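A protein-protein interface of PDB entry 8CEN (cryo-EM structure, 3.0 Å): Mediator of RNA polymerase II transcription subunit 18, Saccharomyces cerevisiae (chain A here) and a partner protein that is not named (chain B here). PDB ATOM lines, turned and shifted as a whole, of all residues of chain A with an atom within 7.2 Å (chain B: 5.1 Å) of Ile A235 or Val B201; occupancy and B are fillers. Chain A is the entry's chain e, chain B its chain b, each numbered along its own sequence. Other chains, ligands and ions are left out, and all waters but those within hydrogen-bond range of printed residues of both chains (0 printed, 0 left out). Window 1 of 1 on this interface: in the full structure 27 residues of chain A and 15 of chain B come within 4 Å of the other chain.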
ATOM      1  N   PHE A 213       8.374   6.186   7.782  1.00  0.00           N
ATOM      2  CA  PHE A 213       8.786   7.439   8.398  1.00  0.00           C
ATOM      3  C   PHE A 213       9.047   8.447   7.288  1.00  0.00           C
ATOM      4  O   PHE A 213       9.135   8.093   6.110  1.00  0.00           O
ATOM      5  CB  PHE A 213      10.020   7.249   9.292  1.00  0.00           C
ATOM      6  CG  PHE A 213      11.328   7.254   8.545  1.00  0.00           C
ATOM      7  CD1 PHE A 213      11.767   6.114   7.893  1.00  0.00           C
ATOM      8  CD2 PHE A 213      12.133   8.385   8.527  1.00  0.00           C
ATOM      9  CE1 PHE A 213      12.971   6.108   7.214  1.00  0.00           C
ATOM     10  CE2 PHE A 213      13.336   8.385   7.847  1.00  0.00           C
ATOM     11  CZ  PHE A 213      13.755   7.245   7.190  1.00  0.00           C
ATOM     12  N   GLN A 214       9.162   9.713   7.680  1.00  0.00           N
ATOM     13  CA  GLN A 214       9.445  10.771   6.725  1.00  0.00           C
ATOM     14  C   GLN A 214      10.288  11.846   7.393  1.00  0.00           C
ATOM     15  O   GLN A 214      10.181  12.088   8.598  1.00  0.00           O
ATOM     16  CB  GLN A 214       8.155  11.375   6.156  1.00  0.00           C
ATOM     17  CG  GLN A 214       7.257  12.025   7.192  1.00  0.00           C
ATOM     18  CD  GLN A 214       6.045  12.689   6.577  1.00  0.00           C
ATOM     19  OE1 GLN A 214       6.113  13.231   5.474  1.00  0.00           O
ATOM     20  NE2 GLN A 214       4.923  12.642   7.286  1.00  0.00           N
ATOM     21  N   TYR A 215      11.130  12.490   6.590  1.00  0.00           N
ATOM     22  CA  TYR A 215      11.986  13.558   7.078  1.00  0.00           C
ATOM     23  C   TYR A 215      12.040  14.680   6.053  1.00  0.00           C
ATOM     24  O   TYR A 215      12.066  14.433   4.844  1.00  0.00           O
ATOM     25  CB  TYR A 215      13.404  13.046   7.394  1.00  0.00           C
ATOM     26  CG  TYR A 215      14.181  12.518   6.204  1.00  0.00           C
ATOM     27  CD1 TYR A 215      14.069  11.191   5.812  1.00  0.00           C
ATOM     28  CD2 TYR A 215      15.049  13.341   5.492  1.00  0.00           C
ATOM     29  CE1 TYR A 215      14.782  10.702   4.735  1.00  0.00           C
ATOM     30  CE2 TYR A 215      15.762  12.861   4.411  1.00  0.00           C
ATOM     31  CZ  TYR A 215      15.628  11.542   4.039  1.00  0.00           C
ATOM     32  OH  TYR A 215      16.338  11.061   2.963  1.00  0.00           O
ATOM     33  N   LEU A 216      12.050  15.909   6.553  1.00  0.00           N
ATOM     34  CA  LEU A 216      12.264  17.094   5.739  1.00  0.00           C
ATOM     35  C   LEU A 216      13.692  17.577   5.946  1.00  0.00           C
ATOM     36  O   LEU A 216      14.113  17.817   7.081  1.00  0.00           O
ATOM     37  CB  LEU A 216      11.278  18.203   6.106  1.00  0.00           C
ATOM     38  CG  LEU A 216      11.561  19.562   5.465  1.00  0.00           C
ATOM     39  CD1 LEU A 216      11.272  19.526   3.972  1.00  0.00           C
ATOM     40  CD2 LEU A 216      10.769  20.666   6.148  1.00  0.00           C
ATOM     41  N   THR A 217      14.433  17.706   4.853  1.00  0.00           N
ATOM     42  CA  THR A 217      15.788  18.230   4.895  1.00  0.00           C
ATOM     43  C   THR A 217      15.827  19.590   4.208  1.00  0.00           C
ATOM     44  O   THR A 217      15.244  19.771   3.136  1.00  0.00           O
ATOM     45  CB  THR A 217      16.784  17.246   4.264  1.00  0.00           C
ATOM     46  OG1 THR A 217      18.092  17.826   4.250  1.00  0.00           O
ATOM     47  CG2 THR A 217      16.377  16.825   2.859  1.00  0.00           C
ATOM     48  N   ILE A 218      16.463  20.554   4.866  1.00  0.00           N
ATOM     49  CA  ILE A 218      16.608  21.911   4.346  1.00  0.00           C
ATOM     50  C   ILE A 218      18.084  22.270   4.388  1.00  0.00           C
ATOM     51  O   ILE A 218      18.723  22.150   5.437  1.00  0.00           O
ATOM     52  CB  ILE A 218      15.786  22.936   5.153  1.00  0.00           C
ATOM     53  CG1 ILE A 218      14.320  22.514   5.251  1.00  0.00           C
ATOM     54  CG2 ILE A 218      15.880  24.310   4.514  1.00  0.00           C
ATOM     55  CD1 ILE A 218      13.513  23.359   6.208  1.00  0.00           C
ATOM     56  N   GLN A 233      23.122  20.459   5.009  1.00  0.00           N
ATOM     57  CA  GLN A 233      21.697  20.417   5.309  1.00  0.00           C
ATOM     58  C   GLN A 233      21.418  20.071   6.768  1.00  0.00           C
ATOM     59  O   GLN A 233      22.236  19.468   7.466  1.00  0.00           O
ATOM     60  CB  GLN A 233      20.971  19.420   4.392  1.00  0.00           C
ATOM     61  CG  GLN A 233      21.293  17.949   4.642  1.00  0.00           C
ATOM     62  CD  GLN A 233      22.547  17.476   3.926  1.00  0.00           C
ATOM     63  OE1 GLN A 233      23.366  18.278   3.480  1.00  0.00           O
ATOM     64  NE2 GLN A 233      22.693  16.163   3.801  1.00  0.00           N
ATOM     65  N   LYS A 234      20.237  20.500   7.213  1.00  0.00           N
ATOM     66  CA  LYS A 234      19.575  20.064   8.432  1.00  0.00           C
ATOM     67  C   LYS A 234      18.476  19.070   8.075  1.00  0.00           C
ATOM     68  O   LYS A 234      17.866  19.157   7.006  1.00  0.00           O
ATOM     69  CB  LYS A 234      18.948  21.247   9.171  1.00  0.00           C
ATOM     70  CG  LYS A 234      19.892  22.294   9.727  1.00  0.00           C
ATOM     71  CD  LYS A 234      20.611  21.786  10.955  1.00  0.00           C
ATOM     72  CE  LYS A 234      21.464  22.873  11.574  1.00  0.00           C
ATOM     73  NZ  LYS A 234      20.635  23.960  12.160  1.00  0.00           N
ATOM     74  N   ILE A 235      18.215  18.133   8.986  1.00  0.00           N
ATOM     75  CA  ILE A 235      17.207  17.095   8.787  1.00  0.00           C
ATOM     76  C   ILE A 235      16.289  17.062  10.003  1.00  0.00           C
ATOM     77  O   ILE A 235      16.764  16.984  11.141  1.00  0.00           O
ATOM     78  CB  ILE A 235      17.852  15.713   8.559  1.00  0.00           C
ATOM     79  CG1 ILE A 235      18.714  15.714   7.295  1.00  0.00           C
ATOM     80  CG2 ILE A 235      16.791  14.634   8.452  1.00  0.00           C
ATOM     81  CD1 ILE A 235      19.504  14.443   7.091  1.00  0.00           C
ATOM     82  N   TRP A 236      14.976  17.113   9.765  1.00  0.00           N
ATOM     83  CA  TRP A 236      13.971  16.956  10.809  1.00  0.00           C
ATOM     84  C   TRP A 236      13.081  15.768  10.477  1.00  0.00           C
ATOM     85  O   TRP A 236      12.645  15.613   9.335  1.00  0.00           O
ATOM     86  CB  TRP A 236      13.087  18.201  10.946  1.00  0.00           C
ATOM     87  CG  TRP A 236      13.785  19.417  11.442  1.00  0.00           C
ATOM     88  CD1 TRP A 236      13.913  19.819  12.738  1.00  0.00           C
ATOM     89  CD2 TRP A 236      14.418  20.421  10.646  1.00  0.00           C
ATOM     90  NE1 TRP A 236      14.607  21.002  12.800  1.00  0.00           N
ATOM     91  CE2 TRP A 236      14.926  21.394  11.526  1.00  0.00           C
ATOM     92  CE3 TRP A 236      14.612  20.587   9.272  1.00  0.00           C
ATOM     93  CZ2 TRP A 236      15.616  22.513  11.078  1.00  0.00           C
ATOM     94  CZ3 TRP A 236      15.297  21.699   8.830  1.00  0.00           C
ATOM     95  CH2 TRP A 236      15.785  22.651   9.730  1.00  0.00           C
ATOM     96  N   GLN A 237      12.792  14.935  11.473  1.00  0.00           N
ATOM     97  CA  GLN A 237      11.853  13.837  11.284  1.00  0.00           C
ATOM     98  C   GLN A 237      10.441  14.328  11.575  1.00  0.00           C
ATOM     99  O   GLN A 237      10.198  14.951  12.613  1.00  0.00           O
ATOM    100  CB  GLN A 237      12.199  12.652  12.185  1.00  0.00           C
ATOM    101  CG  GLN A 237      11.267  11.462  12.010  1.00  0.00           C
ATOM    102  CD  GLN A 237      11.531  10.365  13.018  1.00  0.00           C
ATOM    103  OE1 GLN A 237      12.475  10.444  13.797  1.00  0.00           O
ATOM    104  NE2 GLN A 237      10.709   9.323  12.990  1.00  0.00           N
ATOM    105  N   SER A 244      11.420  16.408  15.285  1.00  0.00           N
ATOM    106  CA  SER A 244      12.667  16.203  16.010  1.00  0.00           C
ATOM    107  C   SER A 244      13.839  16.535  15.101  1.00  0.00           C
ATOM    108  O   SER A 244      13.928  16.013  13.986  1.00  0.00           O
ATOM    109  CB  SER A 244      12.782  14.760  16.516  1.00  0.00           C
ATOM    110  OG  SER A 244      14.056  14.520  17.090  1.00  0.00           O
ATOM    111  N   GLN A 245      14.737  17.393  15.583  1.00  0.00           N
ATOM    112  CA  GLN A 245      15.928  17.782  14.830  1.00  0.00           C
ATOM    113  C   GLN A 245      16.949  16.658  14.953  1.00  0.00           C
ATOM    114  O   GLN A 245      17.558  16.463  16.008  1.00  0.00           O
ATOM    115  CB  GLN A 245      16.478  19.107  15.348  1.00  0.00           C
ATOM    116  CG  GLN A 245      17.872  19.470  14.859  1.00  0.00           C
ATOM    117  CD  GLN A 245      17.888  19.973  13.432  1.00  0.00           C
ATOM    118  OE1 GLN A 245      18.069  19.203  12.490  1.00  0.00           O
ATOM    119  NE2 GLN A 245      17.711  21.278  13.266  1.00  0.00           N
ATOM    120  N   ILE A 246      17.113  15.890  13.874  1.00  0.00           N
ATOM    121  CA  ILE A 246      18.070  14.788  13.882  1.00  0.00           C
ATOM    122  C   ILE A 246      19.498  15.317  13.872  1.00  0.00           C
ATOM    123  O   ILE A 246      20.355  14.849  14.632  1.00  0.00           O
ATOM    124  CB  ILE A 246      17.795  13.847  12.697  1.00  0.00           C
ATOM    125  CG1 ILE A 246      16.372  13.295  12.790  1.00  0.00           C
ATOM    126  CG2 ILE A 246      18.806  12.714  12.661  1.00  0.00           C
ATOM    127  CD1 ILE A 246      16.062  12.603  14.100  1.00  0.00           C
ATOM    128  N   THR A 247      19.777  16.307  13.023  1.00  0.00           N
ATOM    129  CA  THR A 247      21.078  16.977  13.006  1.00  0.00           C
ATOM    130  C   THR A 247      21.087  18.055  14.091  1.00  0.00           C
ATOM    131  O   THR A 247      21.000  19.257  13.833  1.00  0.00           O
ATOM    132  CB  THR A 247      21.363  17.560  11.629  1.00  0.00           C
ATOM    133  OG1 THR A 247      20.364  18.535  11.310  1.00  0.00           O
ATOM    134  CG2 THR A 247      21.352  16.469  10.573  1.00  0.00           C
ATOM    135  N   SER A 248      21.200  17.592  15.334  1.00  0.00           N
ATOM    136  CA  SER A 248      21.054  18.469  16.488  1.00  0.00           C
ATOM    137  C   SER A 248      22.298  19.330  16.662  1.00  0.00           C
ATOM    138  O   SER A 248      23.390  18.816  16.928  1.00  0.00           O
ATOM    139  CB  SER A 248      20.794  17.643  17.745  1.00  0.00           C
ATOM    140  OG  SER A 248      20.548  18.480  18.862  1.00  0.00           O
ATOM    141  N   GLY A 250      24.000  21.150  14.492  1.00  0.00           N
ATOM    142  CA  GLY A 250      25.007  21.180  13.446  1.00  0.00           C
ATOM    143  C   GLY A 250      24.427  20.793  12.105  1.00  0.00           C
ATOM    144  O   GLY A 250      23.321  20.255  12.009  1.00  0.00           O
ATOM    145  N   PHE A 251      25.221  21.045  11.070  1.00  0.00           N
ATOM    146  CA  PHE A 251      24.843  20.786   9.689  1.00  0.00           C
ATOM    147  C   PHE A 251      25.579  19.554   9.177  1.00  0.00           C
ATOM    148  O   PHE A 251      26.766  19.362   9.470  1.00  0.00           O
ATOM    149  CB  PHE A 251      25.175  21.975   8.780  1.00  0.00           C
ATOM    150  CG  PHE A 251      24.339  23.201   9.019  1.00  0.00           C
ATOM    151  CD1 PHE A 251      24.594  24.041  10.093  1.00  0.00           C
ATOM    152  CD2 PHE A 251      23.304  23.524   8.155  1.00  0.00           C
ATOM    153  CE1 PHE A 251      23.833  25.177  10.301  1.00  0.00           C
ATOM    154  CE2 PHE A 251      22.536  24.653   8.361  1.00  0.00           C
ATOM    155  CZ  PHE A 251      22.799  25.481   9.435  1.00  0.00           C
ATOM    156  N   LEU A 252      24.873  18.723   8.408  1.00  0.00           N
ATOM    157  CA  LEU A 252      25.460  17.549   7.778  1.00  0.00           C
ATOM    158  C   LEU A 252      25.970  17.903   6.386  1.00  0.00           C
ATOM    159  O   LEU A 252      25.312  18.631   5.636  1.00  0.00           O
ATOM    160  CB  LEU A 252      24.434  16.416   7.694  1.00  0.00           C
ATOM    161  CG  LEU A 252      24.853  15.124   6.987  1.00  0.00           C
ATOM    162  CD1 LEU A 252      25.717  14.279   7.903  1.00  0.00           C
ATOM    163  CD2 LEU A 252      23.638  14.340   6.523  1.00  0.00           C
ATOM    164  N   SER A 295      25.288   2.156   8.223  1.00  0.00           N
ATOM    165  CA  SER A 295      24.483   3.366   8.329  1.00  0.00           C
ATOM    166  C   SER A 295      23.790   3.695   7.013  1.00  0.00           C
ATOM    167  O   SER A 295      22.614   4.072   7.004  1.00  0.00           O
ATOM    168  CB  SER A 295      25.353   4.537   8.784  1.00  0.00           C
ATOM    169  OG  SER A 295      26.026   4.230   9.991  1.00  0.00           O
ATOM    170  N   PHE B 196      27.035  15.971  16.273  1.00  0.00           N
ATOM    171  CA  PHE B 196      26.259  14.739  16.251  1.00  0.00           C
ATOM    172  C   PHE B 196      27.126  13.640  15.650  1.00  0.00           C
ATOM    173  O   PHE B 196      28.338  13.804  15.478  1.00  0.00           O
ATOM    174  CB  PHE B 196      24.945  14.938  15.480  1.00  0.00           C
ATOM    175  CG  PHE B 196      25.119  15.584  14.128  1.00  0.00           C
ATOM    176  CD1 PHE B 196      25.490  14.834  13.022  1.00  0.00           C
ATOM    177  CD2 PHE B 196      24.897  16.939  13.965  1.00  0.00           C
ATOM    178  CE1 PHE B 196      25.645  15.427  11.783  1.00  0.00           C
ATOM    179  CE2 PHE B 196      25.052  17.536  12.729  1.00  0.00           C
ATOM    180  CZ  PHE B 196      25.425  16.779  11.638  1.00  0.00           C
ATOM    181  N   ASN B 197      26.498  12.516  15.323  1.00  0.00           N
ATOM    182  CA  ASN B 197      27.165  11.405  14.659  1.00  0.00           C
ATOM    183  C   ASN B 197      26.648  11.314  13.230  1.00  0.00           C
ATOM    184  O   ASN B 197      25.438  11.170  13.011  1.00  0.00           O
ATOM    185  CB  ASN B 197      26.930  10.095  15.409  1.00  0.00           C
ATOM    186  CG  ASN B 197      27.813   8.969  14.907  1.00  0.00           C
ATOM    187  OD1 ASN B 197      28.785   9.200  14.188  1.00  0.00           O
ATOM    188  ND2 ASN B 197      27.477   7.741  15.284  1.00  0.00           N
ATOM    189  N   VAL B 198      27.570  11.402  12.266  1.00  0.00           N
ATOM    190  CA  VAL B 198      27.210  11.284  10.855  1.00  0.00           C
ATOM    191  C   VAL B 198      26.633   9.904  10.572  1.00  0.00           C
ATOM    192  O   VAL B 198      25.659   9.762   9.821  1.00  0.00           O
ATOM    193  CB  VAL B 198      28.437  11.586   9.972  1.00  0.00           C
ATOM    194  CG1 VAL B 198      28.104  11.423   8.495  1.00  0.00           C
ATOM    195  CG2 VAL B 198      28.960  12.985  10.253  1.00  0.00           C
ATOM    196  N   ASP B 199      27.216   8.871  11.188  1.00  0.00           N
ATOM    197  CA  ASP B 199      26.703   7.514  11.037  1.00  0.00           C
ATOM    198  C   ASP B 199      25.288   7.386  11.590  1.00  0.00           C
ATOM    199  O   ASP B 199      24.432   6.752  10.969  1.00  0.00           O
ATOM    200  CB  ASP B 199      27.638   6.521  11.726  1.00  0.00           C
ATOM    201  CG  ASP B 199      28.995   6.437  11.055  1.00  0.00           C
ATOM    202  OD1 ASP B 199      29.067   6.655   9.828  1.00  0.00           O
ATOM    203  OD2 ASP B 199      29.988   6.151  11.756  1.00  0.00           O
ATOM    204  N   ASP B 200      25.019   8.001  12.744  1.00  0.00           N
ATOM    205  CA  ASP B 200      23.682   7.922  13.328  1.00  0.00           C
ATOM    206  C   ASP B 200      22.654   8.671  12.485  1.00  0.00           C
ATOM    207  O   ASP B 200      21.535   8.181  12.283  1.00  0.00           O
ATOM    208  CB  ASP B 200      23.701   8.462  14.756  1.00  0.00           C
ATOM    209  CG  ASP B 200      24.178   7.434  15.761  1.00  0.00           C
ATOM    210  OD1 ASP B 200      24.454   6.286  15.353  1.00  0.00           O
ATOM    211  OD2 ASP B 200      24.278   7.773  16.958  1.00  0.00           O
ATOM    212  N   VAL B 201      23.021   9.851  11.974  1.00  0.00           N
ATOM    213  CA  VAL B 201      22.098  10.618  11.139  1.00  0.00           C
ATOM    214  C   VAL B 201      21.813   9.891   9.829  1.00  0.00           C
ATOM    215  O   VAL B 201      20.661   9.814   9.387  1.00  0.00           O
ATOM    216  CB  VAL B 201      22.641  12.039  10.905  1.00  0.00           C
ATOM    217  CG1 VAL B 201      21.745  12.806   9.949  1.00  0.00           C
ATOM    218  CG2 VAL B 201      22.710  12.780  12.222  1.00  0.00           C
ATOM    219  N   LEU B 202      22.843   9.318   9.200  1.00  0.00           N
ATOM    220  CA  LEU B 202      22.613   8.569   7.967  1.00  0.00           C
ATOM    221  C   LEU B 202      21.853   7.272   8.221  1.00  0.00           C
ATOM    222  O   LEU B 202      21.065   6.842   7.369  1.00  0.00           O
ATOM    223  CB  LEU B 202      23.942   8.282   7.270  1.00  0.00           C
ATOM    224  CG  LEU B 202      24.615   9.488   6.613  1.00  0.00           C
ATOM    225  CD1 LEU B 202      25.759   9.034   5.728  1.00  0.00           C
ATOM    226  CD2 LEU B 202      23.610  10.307   5.816  1.00  0.00           C
ATOM    227  N   LYS B 203      22.058   6.644   9.381  1.00  0.00           N
ATOM    228  CA  LYS B 203      21.324   5.425   9.690  1.00  0.00           C
ATOM    229  C   LYS B 203      19.856   5.738   9.945  1.00  0.00           C
ATOM    230  O   LYS B 203      18.986   4.932   9.597  1.00  0.00           O
ATOM    231  CB  LYS B 203      21.988   4.719  10.879  1.00  0.00           C
ATOM    232  CG  LYS B 203      21.466   3.321  11.231  1.00  0.00           C
ATOM    233  CD  LYS B 203      20.346   3.288  12.256  1.00  0.00           C
ATOM    234  CE  LYS B 203      19.978   1.846  12.570  1.00  0.00           C
ATOM    235  NZ  LYS B 203      18.864   1.731  13.542  1.00  0.00           N
ATOM    236  N   PHE B 204      19.563   6.905  10.525  1.00  0.00           N
ATOM    237  CA  PHE B 204      18.187   7.395  10.544  1.00  0.00           C
ATOM    238  C   PHE B 204      17.670   7.634   9.131  1.00  0.00           C
ATOM    239  O   PHE B 204      16.529   7.287   8.806  1.00  0.00           O
ATOM    240  CB  PHE B 204      18.086   8.689  11.354  1.00  0.00           C
ATOM    241  CG  PHE B 204      16.890   9.527  10.988  1.00  0.00           C
ATOM    242  CD1 PHE B 204      15.620   9.161  11.403  1.00  0.00           C
ATOM    243  CD2 PHE B 204      17.033  10.668  10.207  1.00  0.00           C
ATOM    244  CE1 PHE B 204      14.519   9.917  11.054  1.00  0.00           C
ATOM    245  CE2 PHE B 204      15.935  11.418   9.848  1.00  0.00           C
ATOM    246  CZ  PHE B 204      14.680  11.046  10.276  1.00  0.00           C
ATOM    247  N   THR B 205      18.495   8.264   8.290  1.00  0.00           N
ATOM    248  CA  THR B 205      18.077   8.657   6.947  1.00  0.00           C
ATOM    249  C   THR B 205      17.724   7.446   6.092  1.00  0.00           C
ATOM    250  O   THR B 205      16.838   7.523   5.233  1.00  0.00           O
ATOM    251  CB  THR B 205      19.194   9.481   6.295  1.00  0.00           C
ATOM    252  OG1 THR B 205      19.583  10.538   7.181  1.00  0.00           O
ATOM    253  CG2 THR B 205      18.742  10.092   4.981  1.00  0.00           C
ATOM    254  N   PRO B 211      18.739   8.596  16.382  1.00  0.00           N
ATOM    255  CA  PRO B 211      20.108   8.523  16.905  1.00  0.00           C
ATOM    256  C   PRO B 211      20.102   8.390  18.421  1.00  0.00           C
ATOM    257  O   PRO B 211      19.312   9.031  19.117  1.00  0.00           O
ATOM    258  CB  PRO B 211      20.731   9.851  16.458  1.00  0.00           C
ATOM    259  CG  PRO B 211      19.891  10.301  15.310  1.00  0.00           C
ATOM    260  CD  PRO B 211      18.504   9.831  15.614  1.00  0.00           C
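O of Ser A295 sits close to O of Leu B202, at 3.2 Å. The side-chain hydroxyl (OG) of Ser A295 lies within hydrogen-bond range of the backbone carbonyl oxygen (O) of Asp B199, at 3.1 Å.
Of the printed residues of chain B, Ile A235 touches Val B201, Phe B204 and Thr B205. Of the printed residues of chain A, Asp B199 touches Ser A295. Of the printed residues of chain A, Val B201 touches Ile A235 (3.98 Å), Ile A246 (3.9 Å) and Thr A247 (3.7 Å). Of the printed residues of chain A, Pro B211 touches Ile A246. The nearest printed residue of chain B that does not touch Ile A235 is Leu B202 (6.0 Å).
O of Ile A235 sits at hydrogen-bond distance from N of Ile A246, 3.0 Å away. The backbone carbonyl oxygen (O) of Ile A235 sits close to the side-chain amide oxygen (OE1) of Gln A245, at 2.9 Å. OD1 of Asn B197 sits close to N of Asp B199 (3.4 Å). The side-chain hydroxyl (OG1) of Thr A247 lies within hydrogen-bond range of the backbone NH (N) of Ile A235, 3.2 Å away. The side-chain amide oxygen of Gln A245 is in hydrogen-bond range of the side-chain hydroxyl of Thr A247 (2.7 Å). O of Gln A233 is in hydrogen-bond range of N of Leu A252 (2.9 Å).
Hydrophobic or aromatic side chains of chain A within 4 Å of the printed part of chain B: Phe A213, Tyr A215, Ile A235, Ile A246 and Leu A252. Of the 11 printed residues of chain B, 9 touch a printed residue of chain A. Among the printed residues, no Asp or Glu carboxylate lies within 4 Å of a Lys or Arg side-chain nitrogen of the other chain.
Phe A213 touches Phe B204. CZ of Phe A213 touches O of Thr B205 (3.7 Å). CZ of Phe B204 touches CB of Tyr A215 (3.7 Å). CG2 of Thr B205 touches OH of Tyr A215 (3.3 Å). Ile A235 touches Thr B205 (CD1 to OG1, 3.9 Å). Ile A246 touches Pro B211. Thr A247 touches Phe B196. Val B201 touches Thr A247 (CG1 to CG2, 3.7 Å). CE2 of Phe B196 touches O of Gly A250, 3.3 Å away. Leu A252 touches Val B198 (CD1 to CG1, 3.8 Å).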
